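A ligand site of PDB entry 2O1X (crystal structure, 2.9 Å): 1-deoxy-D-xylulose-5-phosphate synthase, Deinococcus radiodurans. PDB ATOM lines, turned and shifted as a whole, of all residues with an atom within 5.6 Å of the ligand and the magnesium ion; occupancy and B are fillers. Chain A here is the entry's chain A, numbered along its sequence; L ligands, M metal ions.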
ATOM      1  N   SER A  54      23.090 -27.665   2.559  1.00  0.00           N
ATOM      2  CA  SER A  54      23.630 -27.261   1.283  1.00  0.00           C
ATOM      3  C   SER A  54      24.781 -28.161   0.882  1.00  0.00           C
ATOM      4  O   SER A  54      24.960 -28.447  -0.298  1.00  0.00           O
ATOM      5  CB  SER A  54      24.119 -25.818   1.358  1.00  0.00           C
ATOM      6  OG  SER A  54      23.040 -24.909   1.228  1.00  0.00           O
ATOM      7  N   ASP A  79      30.451 -21.109  -5.901  1.00  0.00           N
ATOM      8  CA  ASP A  79      29.704 -19.914  -5.536  1.00  0.00           C
ATOM      9  C   ASP A  79      29.221 -19.977  -4.082  1.00  0.00           C
ATOM     10  O   ASP A  79      28.606 -20.972  -3.670  1.00  0.00           O
ATOM     11  CB  ASP A  79      28.543 -19.703  -6.502  1.00  0.00           C
ATOM     12  CG  ASP A  79      28.045 -18.284  -6.516  1.00  0.00           C
ATOM     13  OD1 ASP A  79      27.217 -17.946  -5.642  1.00  0.00           O
ATOM     14  OD2 ASP A  79      28.410 -17.424  -7.353  1.00  0.00           O
ATOM     15  N   VAL A  80      29.493 -18.908  -3.320  1.00  0.00           N
ATOM     16  CA  VAL A  80      29.330 -18.807  -1.848  1.00  0.00           C
ATOM     17  C   VAL A  80      30.317 -19.692  -1.060  1.00  0.00           C
ATOM     18  O   VAL A  80      31.084 -19.193  -0.235  1.00  0.00           O
ATOM     19  CB  VAL A  80      27.882 -19.030  -1.323  1.00  0.00           C
ATOM     20  CG1 VAL A  80      27.763 -18.543   0.119  1.00  0.00           C
ATOM     21  CG2 VAL A  80      26.889 -18.304  -2.180  1.00  0.00           C
ATOM     22  N   HIS A  82      29.495 -22.369   0.826  1.00  0.00           N
ATOM     23  CA  HIS A  82      28.845 -23.037   1.958  1.00  0.00           C
ATOM     24  C   HIS A  82      28.470 -24.471   1.600  1.00  0.00           C
ATOM     25  O   HIS A  82      28.106 -25.252   2.467  1.00  0.00           O
ATOM     26  CB  HIS A  82      27.594 -22.263   2.369  1.00  0.00           C
ATOM     27  CG  HIS A  82      26.532 -22.251   1.321  1.00  0.00           C
ATOM     28  ND1 HIS A  82      26.780 -21.856   0.016  1.00  0.00           N
ATOM     29  CD2 HIS A  82      25.217 -22.593   1.365  1.00  0.00           C
ATOM     30  CE1 HIS A  82      25.666 -21.956  -0.686  1.00  0.00           C
ATOM     31  NE2 HIS A  82      24.713 -22.401   0.106  1.00  0.00           N
ATOM     32  N   GLN A  83      28.564 -24.825   0.310  1.00  0.00           N
ATOM     33  CA  GLN A  83      28.154 -26.147  -0.106  1.00  0.00           C
ATOM     34  C   GLN A  83      29.315 -27.104  -0.327  1.00  0.00           C
ATOM     35  O   GLN A  83      29.102 -28.237  -0.778  1.00  0.00           O
ATOM     36  CB  GLN A  83      27.321 -26.065  -1.386  1.00  0.00           C
ATOM     37  CG  GLN A  83      28.116 -25.875  -2.678  1.00  0.00           C
ATOM     38  CD  GLN A  83      28.279 -24.407  -3.058  1.00  0.00           C
ATOM     39  OE1 GLN A  83      29.056 -23.676  -2.461  1.00  0.00           O
ATOM     40  NE2 GLN A  83      27.552 -23.984  -4.091  1.00  0.00           N
ATOM     41  N   GLY A 123      32.097 -15.948   0.053  1.00  0.00           N
ATOM     42  CA  GLY A 123      31.321 -15.678   1.253  1.00  0.00           C
ATOM     43  C   GLY A 123      30.066 -14.981   0.770  1.00  0.00           C
ATOM     44  O   GLY A 123      28.971 -15.423   1.081  1.00  0.00           O
ATOM     45  N   HIS A 124      30.253 -13.907   0.002  1.00  0.00           N
ATOM     46  CA  HIS A 124      29.182 -13.255  -0.743  1.00  0.00           C
ATOM     47  C   HIS A 124      28.825 -14.121  -1.956  1.00  0.00           C
ATOM     48  O   HIS A 124      29.676 -14.801  -2.520  1.00  0.00           O
ATOM     49  CB  HIS A 124      29.625 -11.874  -1.196  1.00  0.00           C
ATOM     50  CG  HIS A 124      29.705 -10.864  -0.085  1.00  0.00           C
ATOM     51  ND1 HIS A 124      29.847  -9.508  -0.322  1.00  0.00           N
ATOM     52  CD2 HIS A 124      29.631 -11.014   1.257  1.00  0.00           C
ATOM     53  CE1 HIS A 124      29.871  -8.866   0.831  1.00  0.00           C
ATOM     54  NE2 HIS A 124      29.733  -9.749   1.810  1.00  0.00           N
ATOM     55  N   ALA A 125      27.551 -14.115  -2.348  1.00  0.00           N
ATOM     56  CA  ALA A 125      27.069 -14.976  -3.431  1.00  0.00           C
ATOM     57  C   ALA A 125      27.376 -14.381  -4.789  1.00  0.00           C
ATOM     58  O   ALA A 125      27.805 -13.221  -4.887  1.00  0.00           O
ATOM     59  CB  ALA A 125      25.582 -15.166  -3.285  1.00  0.00           C
ATOM     60  N   ILE A 152      27.431 -23.011  -9.270  1.00  0.00           N
ATOM     61  CA  ILE A 152      26.494 -21.999  -8.771  1.00  0.00           C
ATOM     62  C   ILE A 152      25.089 -22.581  -8.467  1.00  0.00           C
ATOM     63  O   ILE A 152      24.475 -23.252  -9.318  1.00  0.00           O
ATOM     64  CB  ILE A 152      26.425 -20.778  -9.733  1.00  0.00           C
ATOM     65  CG1 ILE A 152      25.650 -19.628  -9.093  1.00  0.00           C
ATOM     66  CG2 ILE A 152      25.812 -21.138 -11.093  1.00  0.00           C
ATOM     67  CD1 ILE A 152      26.106 -18.265  -9.557  1.00  0.00           C
ATOM     68  N   GLY A 153      24.612 -22.331  -7.255  1.00  0.00           N
ATOM     69  CA  GLY A 153      23.255 -22.692  -6.879  1.00  0.00           C
ATOM     70  C   GLY A 153      22.247 -21.750  -7.536  1.00  0.00           C
ATOM     71  O   GLY A 153      22.629 -20.755  -8.172  1.00  0.00           O
ATOM     72  N   ASP A 154      20.955 -22.047  -7.378  1.00  0.00           N
ATOM     73  CA  ASP A 154      19.929 -21.366  -8.144  1.00  0.00           C
ATOM     74  C   ASP A 154      19.549 -19.997  -7.566  1.00  0.00           C
ATOM     75  O   ASP A 154      19.225 -19.068  -8.311  1.00  0.00           O
ATOM     76  CB  ASP A 154      18.720 -22.273  -8.325  1.00  0.00           C
ATOM     77  CG  ASP A 154      18.046 -22.637  -7.020  1.00  0.00           C
ATOM     78  OD1 ASP A 154      16.842 -22.298  -6.909  1.00  0.00           O
ATOM     79  OD2 ASP A 154      18.600 -23.237  -6.073  1.00  0.00           O
ATOM     80  N   GLY A 155      19.616 -19.867  -6.241  1.00  0.00           N
ATOM     81  CA  GLY A 155      19.447 -18.576  -5.575  1.00  0.00           C
ATOM     82  C   GLY A 155      20.577 -17.627  -5.944  1.00  0.00           C
ATOM     83  O   GLY A 155      20.368 -16.436  -6.160  1.00  0.00           O
ATOM     84  N   SER A 156      21.787 -18.164  -6.034  1.00  0.00           N
ATOM     85  CA  SER A 156      22.960 -17.374  -6.403  1.00  0.00           C
ATOM     86  C   SER A 156      22.837 -16.718  -7.769  1.00  0.00           C
ATOM     87  O   SER A 156      23.232 -15.558  -7.955  1.00  0.00           O
ATOM     88  CB  SER A 156      24.187 -18.245  -6.347  1.00  0.00           C
ATOM     89  OG  SER A 156      24.818 -18.029  -5.119  1.00  0.00           O
ATOM     90  N   LEU A 157      22.285 -17.494  -8.695  1.00  0.00           N
ATOM     91  CA  LEU A 157      21.982 -17.069 -10.067  1.00  0.00           C
ATOM     92  C   LEU A 157      21.010 -15.874 -10.106  1.00  0.00           C
ATOM     93  O   LEU A 157      20.930 -15.171 -11.113  1.00  0.00           O
ATOM     94  CB  LEU A 157      21.404 -18.250 -10.848  1.00  0.00           C
ATOM     95  CG  LEU A 157      21.254 -18.169 -12.371  1.00  0.00           C
ATOM     96  CD1 LEU A 157      22.611 -18.132 -13.078  1.00  0.00           C
ATOM     97  CD2 LEU A 157      20.396 -19.334 -12.856  1.00  0.00           C
ATOM     98  N   ASN A 181      23.528 -25.657  -9.797  1.00  0.00           N
ATOM     99  CA  ASN A 181      23.035 -26.511  -8.723  1.00  0.00           C
ATOM    100  C   ASN A 181      21.636 -26.123  -8.265  1.00  0.00           C
ATOM    101  O   ASN A 181      21.475 -25.414  -7.267  1.00  0.00           O
ATOM    102  CB  ASN A 181      24.000 -26.465  -7.541  1.00  0.00           C
ATOM    103  CG  ASN A 181      23.574 -27.383  -6.419  1.00  0.00           C
ATOM    104  OD1 ASN A 181      22.780 -28.284  -6.620  1.00  0.00           O
ATOM    105  ND2 ASN A 181      24.092 -27.150  -5.236  1.00  0.00           N
ATOM    106  N   ASP A 182      20.618 -26.593  -8.988  1.00  0.00           N
ATOM    107  CA  ASP A 182      19.250 -26.106  -8.779  1.00  0.00           C
ATOM    108  C   ASP A 182      18.422 -26.992  -7.856  1.00  0.00           C
ATOM    109  O   ASP A 182      17.877 -27.997  -8.283  1.00  0.00           O
ATOM    110  CB  ASP A 182      18.550 -25.879 -10.141  1.00  0.00           C
ATOM    111  CG  ASP A 182      17.063 -25.465 -10.012  1.00  0.00           C
ATOM    112  OD1 ASP A 182      16.291 -25.809 -10.936  1.00  0.00           O
ATOM    113  OD2 ASP A 182      16.579 -24.819  -9.054  1.00  0.00           O
ATOM    114  N   ASN A 183      18.336 -26.616  -6.590  1.00  0.00           N
ATOM    115  CA  ASN A 183      17.442 -27.291  -5.651  1.00  0.00           C
ATOM    116  C   ASN A 183      16.234 -26.480  -5.272  1.00  0.00           C
ATOM    117  O   ASN A 183      15.567 -26.781  -4.310  1.00  0.00           O
ATOM    118  CB  ASN A 183      18.162 -27.712  -4.381  1.00  0.00           C
ATOM    119  CG  ASN A 183      18.771 -26.554  -3.619  1.00  0.00           C
ATOM    120  OD1 ASN A 183      19.504 -26.779  -2.659  1.00  0.00           O
ATOM    121  ND2 ASN A 183      18.505 -25.305  -4.026  1.00  0.00           N
ATOM    122  N   GLU A 184      15.973 -25.433  -6.055  1.00  0.00           N
ATOM    123  CA  GLU A 184      14.917 -24.440  -5.794  1.00  0.00           C
ATOM    124  C   GLU A 184      14.809 -23.953  -4.322  1.00  0.00           C
ATOM    125  O   GLU A 184      13.747 -23.528  -3.856  1.00  0.00           O
ATOM    126  CB  GLU A 184      13.584 -24.861  -6.391  1.00  0.00           C
ATOM    127  CG  GLU A 184      12.911 -26.032  -5.713  1.00  0.00           C
ATOM    128  CD  GLU A 184      11.731 -26.552  -6.501  1.00  0.00           C
ATOM    129  OE1 GLU A 184      11.459 -26.040  -7.603  1.00  0.00           O
ATOM    130  OE2 GLU A 184      11.089 -27.486  -6.004  1.00  0.00           O
ATOM    131  N   MET A 185      15.931 -24.019  -3.623  1.00  0.00           N
ATOM    132  CA  MET A 185      16.080 -23.317  -2.366  1.00  0.00           C
ATOM    133  C   MET A 185      17.188 -22.274  -2.489  1.00  0.00           C
ATOM    134  O   MET A 185      18.206 -22.488  -3.195  1.00  0.00           O
ATOM    135  CB  MET A 185      16.382 -24.284  -1.223  1.00  0.00           C
ATOM    136  CG  MET A 185      15.289 -25.279  -0.926  1.00  0.00           C
ATOM    137  SD  MET A 185      13.859 -24.496  -0.183  1.00  0.00           S
ATOM    138  CE  MET A 185      12.541 -25.224  -1.170  1.00  0.00           C
ATOM    139  N   SER A 186      16.943 -21.127  -1.828  1.00  0.00           N
ATOM    140  CA  SER A 186      17.970 -20.175  -1.409  1.00  0.00           C
ATOM    141  C   SER A 186      18.309 -20.540   0.040  1.00  0.00           C
ATOM    142  O   SER A 186      18.717 -21.672   0.324  1.00  0.00           O
ATOM    143  CB  SER A 186      17.435 -18.749  -1.524  1.00  0.00           C
ATOM    144  OG  SER A 186      18.467 -17.821  -1.814  1.00  0.00           O
ATOM    145  N   ILE A 187      18.140 -19.624   0.980  1.00  0.00           N
ATOM    146  CA  ILE A 187      18.147 -20.008   2.389  1.00  0.00           C
ATOM    147  C   ILE A 187      16.669 -20.263   2.694  1.00  0.00           C
ATOM    148  O   ILE A 187      16.276 -21.347   3.168  1.00  0.00           O
ATOM    149  CB  ILE A 187      18.784 -18.920   3.303  1.00  0.00           C
ATOM    150  CG1 ILE A 187      20.278 -18.806   3.004  1.00  0.00           C
ATOM    151  CG2 ILE A 187      18.493 -19.220   4.770  1.00  0.00           C
ATOM    152  CD1 ILE A 187      21.108 -18.047   3.999  1.00  0.00           C
ATOM    153  N   ASN A 190      13.560 -20.256  -2.763  1.00  0.00           N
ATOM    154  CA  ASN A 190      14.063 -19.351  -3.790  1.00  0.00           C
ATOM    155  C   ASN A 190      12.957 -18.543  -4.457  1.00  0.00           C
ATOM    156  O   ASN A 190      11.856 -19.037  -4.662  1.00  0.00           O
ATOM    157  CB  ASN A 190      14.875 -20.088  -4.841  1.00  0.00           C
ATOM    158  CG  ASN A 190      15.818 -19.188  -5.592  1.00  0.00           C
ATOM    159  OD1 ASN A 190      16.255 -19.495  -6.693  1.00  0.00           O
ATOM    160  ND2 ASN A 190      16.161 -18.050  -4.984  1.00  0.00           N
ATOM    161  N   LYS A 289      18.051 -30.223  -1.337  1.00  0.00           N
ATOM    162  CA  LYS A 289      18.743 -29.587  -0.207  1.00  0.00           C
ATOM    163  C   LYS A 289      18.532 -30.521   0.967  1.00  0.00           C
ATOM    164  O   LYS A 289      17.376 -30.885   1.292  1.00  0.00           O
ATOM    165  CB  LYS A 289      18.217 -28.161   0.072  1.00  0.00           C
ATOM    166  CG  LYS A 289      19.045 -27.361   1.087  1.00  0.00           C
ATOM    167  CD  LYS A 289      19.440 -25.989   0.520  1.00  0.00           C
ATOM    168  CE  LYS A 289      19.756 -24.950   1.587  1.00  0.00           C
ATOM    169  NZ  LYS A 289      18.518 -24.184   2.007  1.00  0.00           N
ATOM    170  N   HIS A 304      19.655 -25.599   6.925  1.00  0.00           N
ATOM    171  CA  HIS A 304      20.653 -24.833   6.183  1.00  0.00           C
ATOM    172  C   HIS A 304      21.891 -24.511   7.037  1.00  0.00           C
ATOM    173  O   HIS A 304      23.038 -24.659   6.583  1.00  0.00           O
ATOM    174  CB  HIS A 304      20.036 -23.533   5.638  1.00  0.00           C
ATOM    175  CG  HIS A 304      20.989 -22.714   4.829  1.00  0.00           C
ATOM    176  ND1 HIS A 304      21.735 -21.691   5.385  1.00  0.00           N
ATOM    177  CD2 HIS A 304      21.350 -22.788   3.531  1.00  0.00           C
ATOM    178  CE1 HIS A 304      22.507 -21.166   4.443  1.00  0.00           C
ATOM    179  NE2 HIS A 304      22.292 -21.807   3.313  1.00  0.00           N
ATOM    180  N   PRO A 347      16.623  -8.820   0.773  1.00  0.00           N
ATOM    181  CA  PRO A 347      17.365  -9.509  -0.261  1.00  0.00           C
ATOM    182  C   PRO A 347      17.684 -10.899   0.241  1.00  0.00           C
ATOM    183  O   PRO A 347      18.756 -11.103   0.803  1.00  0.00           O
ATOM    184  CB  PRO A 347      18.640  -8.669  -0.405  1.00  0.00           C
ATOM    185  CG  PRO A 347      18.802  -7.931   0.915  1.00  0.00           C
ATOM    186  CD  PRO A 347      17.513  -8.124   1.713  1.00  0.00           C
ATOM    187  N   ALA A 348      16.719 -11.819   0.073  1.00  0.00           N
ATOM    188  CA  ALA A 348      16.879 -13.261   0.378  1.00  0.00           C
ATOM    189  C   ALA A 348      17.042 -13.666   1.859  1.00  0.00           C
ATOM    190  O   ALA A 348      17.259 -14.848   2.149  1.00  0.00           O
ATOM    191  CB  ALA A 348      17.982 -13.874  -0.474  1.00  0.00           C
ATOM    192  N   MET A 349      16.934 -12.718   2.791  1.00  0.00           N
ATOM    193  CA  MET A 349      17.226 -12.996   4.198  1.00  0.00           C
ATOM    194  C   MET A 349      16.063 -12.829   5.192  1.00  0.00           C
ATOM    195  O   MET A 349      16.274 -12.478   6.356  1.00  0.00           O
ATOM    196  CB  MET A 349      18.457 -12.196   4.652  1.00  0.00           C
ATOM    197  CG  MET A 349      19.726 -12.567   3.935  1.00  0.00           C
ATOM    198  SD  MET A 349      20.489 -14.073   4.552  1.00  0.00           S
ATOM    199  CE  MET A 349      19.683 -15.210   3.469  1.00  0.00           C
ATOM    200  N   ILE A 371      18.841 -12.859  -4.057  1.00  0.00           N
ATOM    201  CA  ILE A 371      20.171 -12.435  -3.612  1.00  0.00           C
ATOM    202  C   ILE A 371      20.660 -11.272  -4.467  1.00  0.00           C
ATOM    203  O   ILE A 371      21.675 -11.369  -5.155  1.00  0.00           O
ATOM    204  CB  ILE A 371      21.193 -13.589  -3.588  1.00  0.00           C
ATOM    205  CG1 ILE A 371      20.500 -14.901  -3.201  1.00  0.00           C
ATOM    206  CG2 ILE A 371      22.338 -13.224  -2.633  1.00  0.00           C
ATOM    207  CD1 ILE A 371      21.423 -16.097  -2.915  1.00  0.00           C
ATOM    208  N   GLU A 373      20.941  -7.330  -3.667  1.00  0.00           N
ATOM    209  CA  GLU A 373      20.882  -6.204  -2.740  1.00  0.00           C
ATOM    210  C   GLU A 373      20.628  -4.940  -3.498  1.00  0.00           C
ATOM    211  O   GLU A 373      19.855  -4.092  -3.056  1.00  0.00           O
ATOM    212  CB  GLU A 373      22.207  -6.082  -1.974  1.00  0.00           C
ATOM    213  CG  GLU A 373      22.359  -7.038  -0.795  1.00  0.00           C
ATOM    214  CD  GLU A 373      22.666  -8.492  -1.155  1.00  0.00           C
ATOM    215  OE1 GLU A 373      22.836  -8.836  -2.346  1.00  0.00           O
ATOM    216  OE2 GLU A 373      22.735  -9.323  -0.226  1.00  0.00           O
ATOM    217  N   PHE A 398      26.270  -7.199   3.384  1.00  0.00           N
ATOM    218  CA  PHE A 398      25.631  -7.311   2.088  1.00  0.00           C
ATOM    219  C   PHE A 398      25.112  -5.969   1.621  1.00  0.00           C
ATOM    220  O   PHE A 398      24.875  -5.758   0.434  1.00  0.00           O
ATOM    221  CB  PHE A 398      24.494  -8.324   2.144  1.00  0.00           C
ATOM    222  CG  PHE A 398      24.907  -9.677   2.633  1.00  0.00           C
ATOM    223  CD1 PHE A 398      26.074 -10.279   2.166  1.00  0.00           C
ATOM    224  CD2 PHE A 398      24.140 -10.352   3.556  1.00  0.00           C
ATOM    225  CE1 PHE A 398      26.472 -11.523   2.623  1.00  0.00           C
ATOM    226  CE2 PHE A 398      24.529 -11.593   4.016  1.00  0.00           C
ATOM    227  CZ  PHE A 398      25.703 -12.174   3.550  1.00  0.00           C
ATOM    228  N   ARG A 401      27.113  -4.433  -1.131  1.00  0.00           N
ATOM    229  CA  ARG A 401      26.693  -4.656  -2.495  1.00  0.00           C
ATOM    230  C   ARG A 401      25.822  -3.552  -3.090  1.00  0.00           C
ATOM    231  O   ARG A 401      25.543  -3.558  -4.285  1.00  0.00           O
ATOM    232  CB  ARG A 401      25.987  -5.989  -2.608  1.00  0.00           C
ATOM    233  CG  ARG A 401      26.955  -7.115  -2.743  1.00  0.00           C
ATOM    234  CD  ARG A 401      27.597  -7.225  -4.121  1.00  0.00           C
ATOM    235  NE  ARG A 401      28.397  -8.437  -4.225  1.00  0.00           N
ATOM    236  CZ  ARG A 401      27.905  -9.648  -4.476  1.00  0.00           C
ATOM    237  NH1 ARG A 401      26.612  -9.803  -4.684  1.00  0.00           N
ATOM    238  NH2 ARG A 401      28.711 -10.701  -4.511  1.00  0.00           N
ATOM    239  N   HIS A 434      32.446 -11.801   5.908  1.00  0.00           N
ATOM    240  CA  HIS A 434      31.146 -11.497   6.511  1.00  0.00           C
ATOM    241  C   HIS A 434      31.096 -10.464   7.585  1.00  0.00           C
ATOM    242  O   HIS A 434      29.999  -9.989   7.898  1.00  0.00           O
ATOM    243  CB  HIS A 434      30.506 -12.761   7.055  1.00  0.00           C
ATOM    244  CG  HIS A 434      29.724 -13.505   6.031  1.00  0.00           C
ATOM    245  ND1 HIS A 434      30.325 -14.178   4.991  1.00  0.00           N
ATOM    246  CD2 HIS A 434      28.394 -13.674   5.882  1.00  0.00           C
ATOM    247  CE1 HIS A 434      29.392 -14.752   4.251  1.00  0.00           C
ATOM    248  NE2 HIS A 434      28.210 -14.456   4.764  1.00  0.00           N
HETATM  249  N1  LIG L   1      23.723 -11.843   0.148  1.00  0.00           N
HETATM  250  C1  LIG L   1      24.929 -11.920  -0.408  1.00  0.00           C
HETATM  251  C2  LIG L   1      25.436 -10.779  -1.286  1.00  0.00           C
HETATM  252  N2  LIG L   1      25.705 -13.003  -0.183  1.00  0.00           N
HETATM  253  C3  LIG L   1      25.290 -14.017   0.582  1.00  0.00           C
HETATM  254  N3  LIG L   1      26.096 -15.055   0.765  1.00  0.00           N
HETATM  255  C4  LIG L   1      24.019 -13.958   1.154  1.00  0.00           C
HETATM  256  C5  LIG L   1      23.272 -12.813   0.903  1.00  0.00           C
HETATM  257  C6  LIG L   1      23.362 -14.985   2.077  1.00  0.00           C
HETATM  258  N4  LIG L   1      23.357 -16.370   1.578  1.00  0.00           N
HETATM  259  C7  LIG L   1      24.350 -17.229   1.909  1.00  0.00           C
HETATM  260  S1  LIG L   1      23.955 -18.765   1.117  1.00  0.00           S
HETATM  261  C8  LIG L   1      22.506 -18.202   0.438  1.00  0.00           C
HETATM  262  C9  LIG L   1      22.353 -16.866   0.798  1.00  0.00           C
HETATM  263  C10 LIG L   1      21.127 -16.090   0.331  1.00  0.00           C
HETATM  264  C11 LIG L   1      21.594 -19.088  -0.389  1.00  0.00           C
HETATM  265  C12 LIG L   1      22.348 -19.662  -1.563  1.00  0.00           C
HETATM  266  O1  LIG L   1      21.377 -20.130  -2.451  1.00  0.00           O
HETATM  267  P1  LIG L   1      21.856 -21.197  -3.454  1.00  0.00           P
HETATM  268  O2  LIG L   1      20.520 -21.727  -4.234  1.00  0.00           O
HETATM  269  O3  LIG L   1      22.943 -20.733  -4.343  1.00  0.00           O
HETATM  270  O4  LIG L   1      22.532 -22.345  -2.501  1.00  0.00           O
HETATM  271  P2  LIG L   1      21.870 -23.654  -1.837  1.00  0.00           P
HETATM  272  O5  LIG L   1      21.311 -23.256  -0.346  1.00  0.00           O
HETATM  273  O6  LIG L   1      20.600 -24.127  -2.775  1.00  0.00           O
HETATM  274  O7  LIG L   1      22.862 -24.723  -1.724  1.00  0.00           O
HETATM  275 MG    MG M   1      19.860 -23.843  -4.536  1.00  0.00          MG
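A ring nitrogen (NE2) of His 82 sits at hydrogen-bond distance from an oxygen (O4) of the ligand, 3.4 Å away.
O3 of the ligand is in hydrogen-bond range of OG of Ser 156, at 3.4 Å.
OG of Ser 54 is in hydrogen-bond range of O5 of the ligand, 2.9 Å away.
N of Gly 155 lies close to O2 of the ligand.
N of Asp 154 sits close to O2 of the ligand (3.2 Å).
An oxygen (O5) of the ligand lies within salt-bridge range of the side-chain amino group (NZ) of Lys 289 (3.8 Å).
N of Ala 125 is in hydrogen-bond range of N2 of the ligand (3.1 Å).
N of Ser 156 sits at hydrogen-bond distance from O3 of the ligand.
O of Gly 123 is in hydrogen-bond range of N3 of the ligand, at 2.9 Å.
A nitrogen (N1) of the ligand is in hydrogen-bond range of the side-chain carboxylate (OE2) of Glu 373 (2.7 Å).
The backbone NH (N) of Gly 123 sits at hydrogen-bond distance from the backbone carbonyl oxygen (O) of Val 80 (3.4 Å).
The guanidinium group (NH2) of Arg 401 sits at hydrogen-bond distance from the backbone carbonyl oxygen (O) of Ala 125 (2.7 Å).
The backbone NH (N) of Asn 181 is in hydrogen-bond range of the backbone carbonyl oxygen (O) of Ile 152.
The side-chain amino group of Lys 289 is in hydrogen-bond range of the backbone carbonyl oxygen of Ser 186.
NE2 of His 82 lies close to OG of Ser 54 (3.2 Å).
The backbone carbonyl oxygen (O) of Asn 181 sits at hydrogen-bond distance from the backbone NH (N) of Asp 154 (3.4 Å).
OD1 of Asp 79 sits at hydrogen-bond distance from OG of Ser 156, at 2.5 Å.
The side-chain carboxylate of Asp 154 sits close to the backbone NH of Glu 184.
The magnesium ion is bound by an oxygen (O6) of the ligand, 1.9 Å away.
The magnesium ion is bound by ND2 of Asn 183.
OD2 of Asp 154 binds the magnesium ion (2.1 Å).
O2 of the ligand is bound to the magnesium ion.
The magnesium ion is bound by the backbone carbonyl oxygen (O) of Met 185 (2.5 Å).
Asn 181 touches the magnesium ion.
Of the 32 residues printed, 4 come within 4 Å of the magnesium ion.
The backbone carbonyl oxygen (O) of Ser 186 lies close to an oxygen (O5) of the ligand, at 3.1 Å.
Merely in contact with the ligand: Val 80 (3.9 Å), His 124 (3.5 Å), Gly 153 (3.2 Å), Ile 187 (3.5 Å), His 304 (3.9 Å), Ala 348 (3.9 Å), Met 349 (3.6 Å), Ile 371 (3.3 Å), Phe 398 (3.3 Å) and Arg 401 (3.7 Å).
Hydrophobic or aromatic side chains within 4 Å of the ligand: Val 80, His 82, Ala 125, Ile 187, His 304, Ala 348, Met 349, Ile 371 and Phe 398.
22 residues have an atom within 4 Å of the ligand: Ser 54, Val 80, His 82, Gly 123, His 124, Ala 125, Gly 153, Asp 154, Gly 155, Ser 156, Asn 183, Met 185, Ser 186, Ile 187, Lys 289, His 304, Ala 348, Met 349, Ile 371, Glu 373, Phe 398 and Arg 401.
The nearest printed residue that does not touch the ligand is Asn 181 (4.4 Å).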
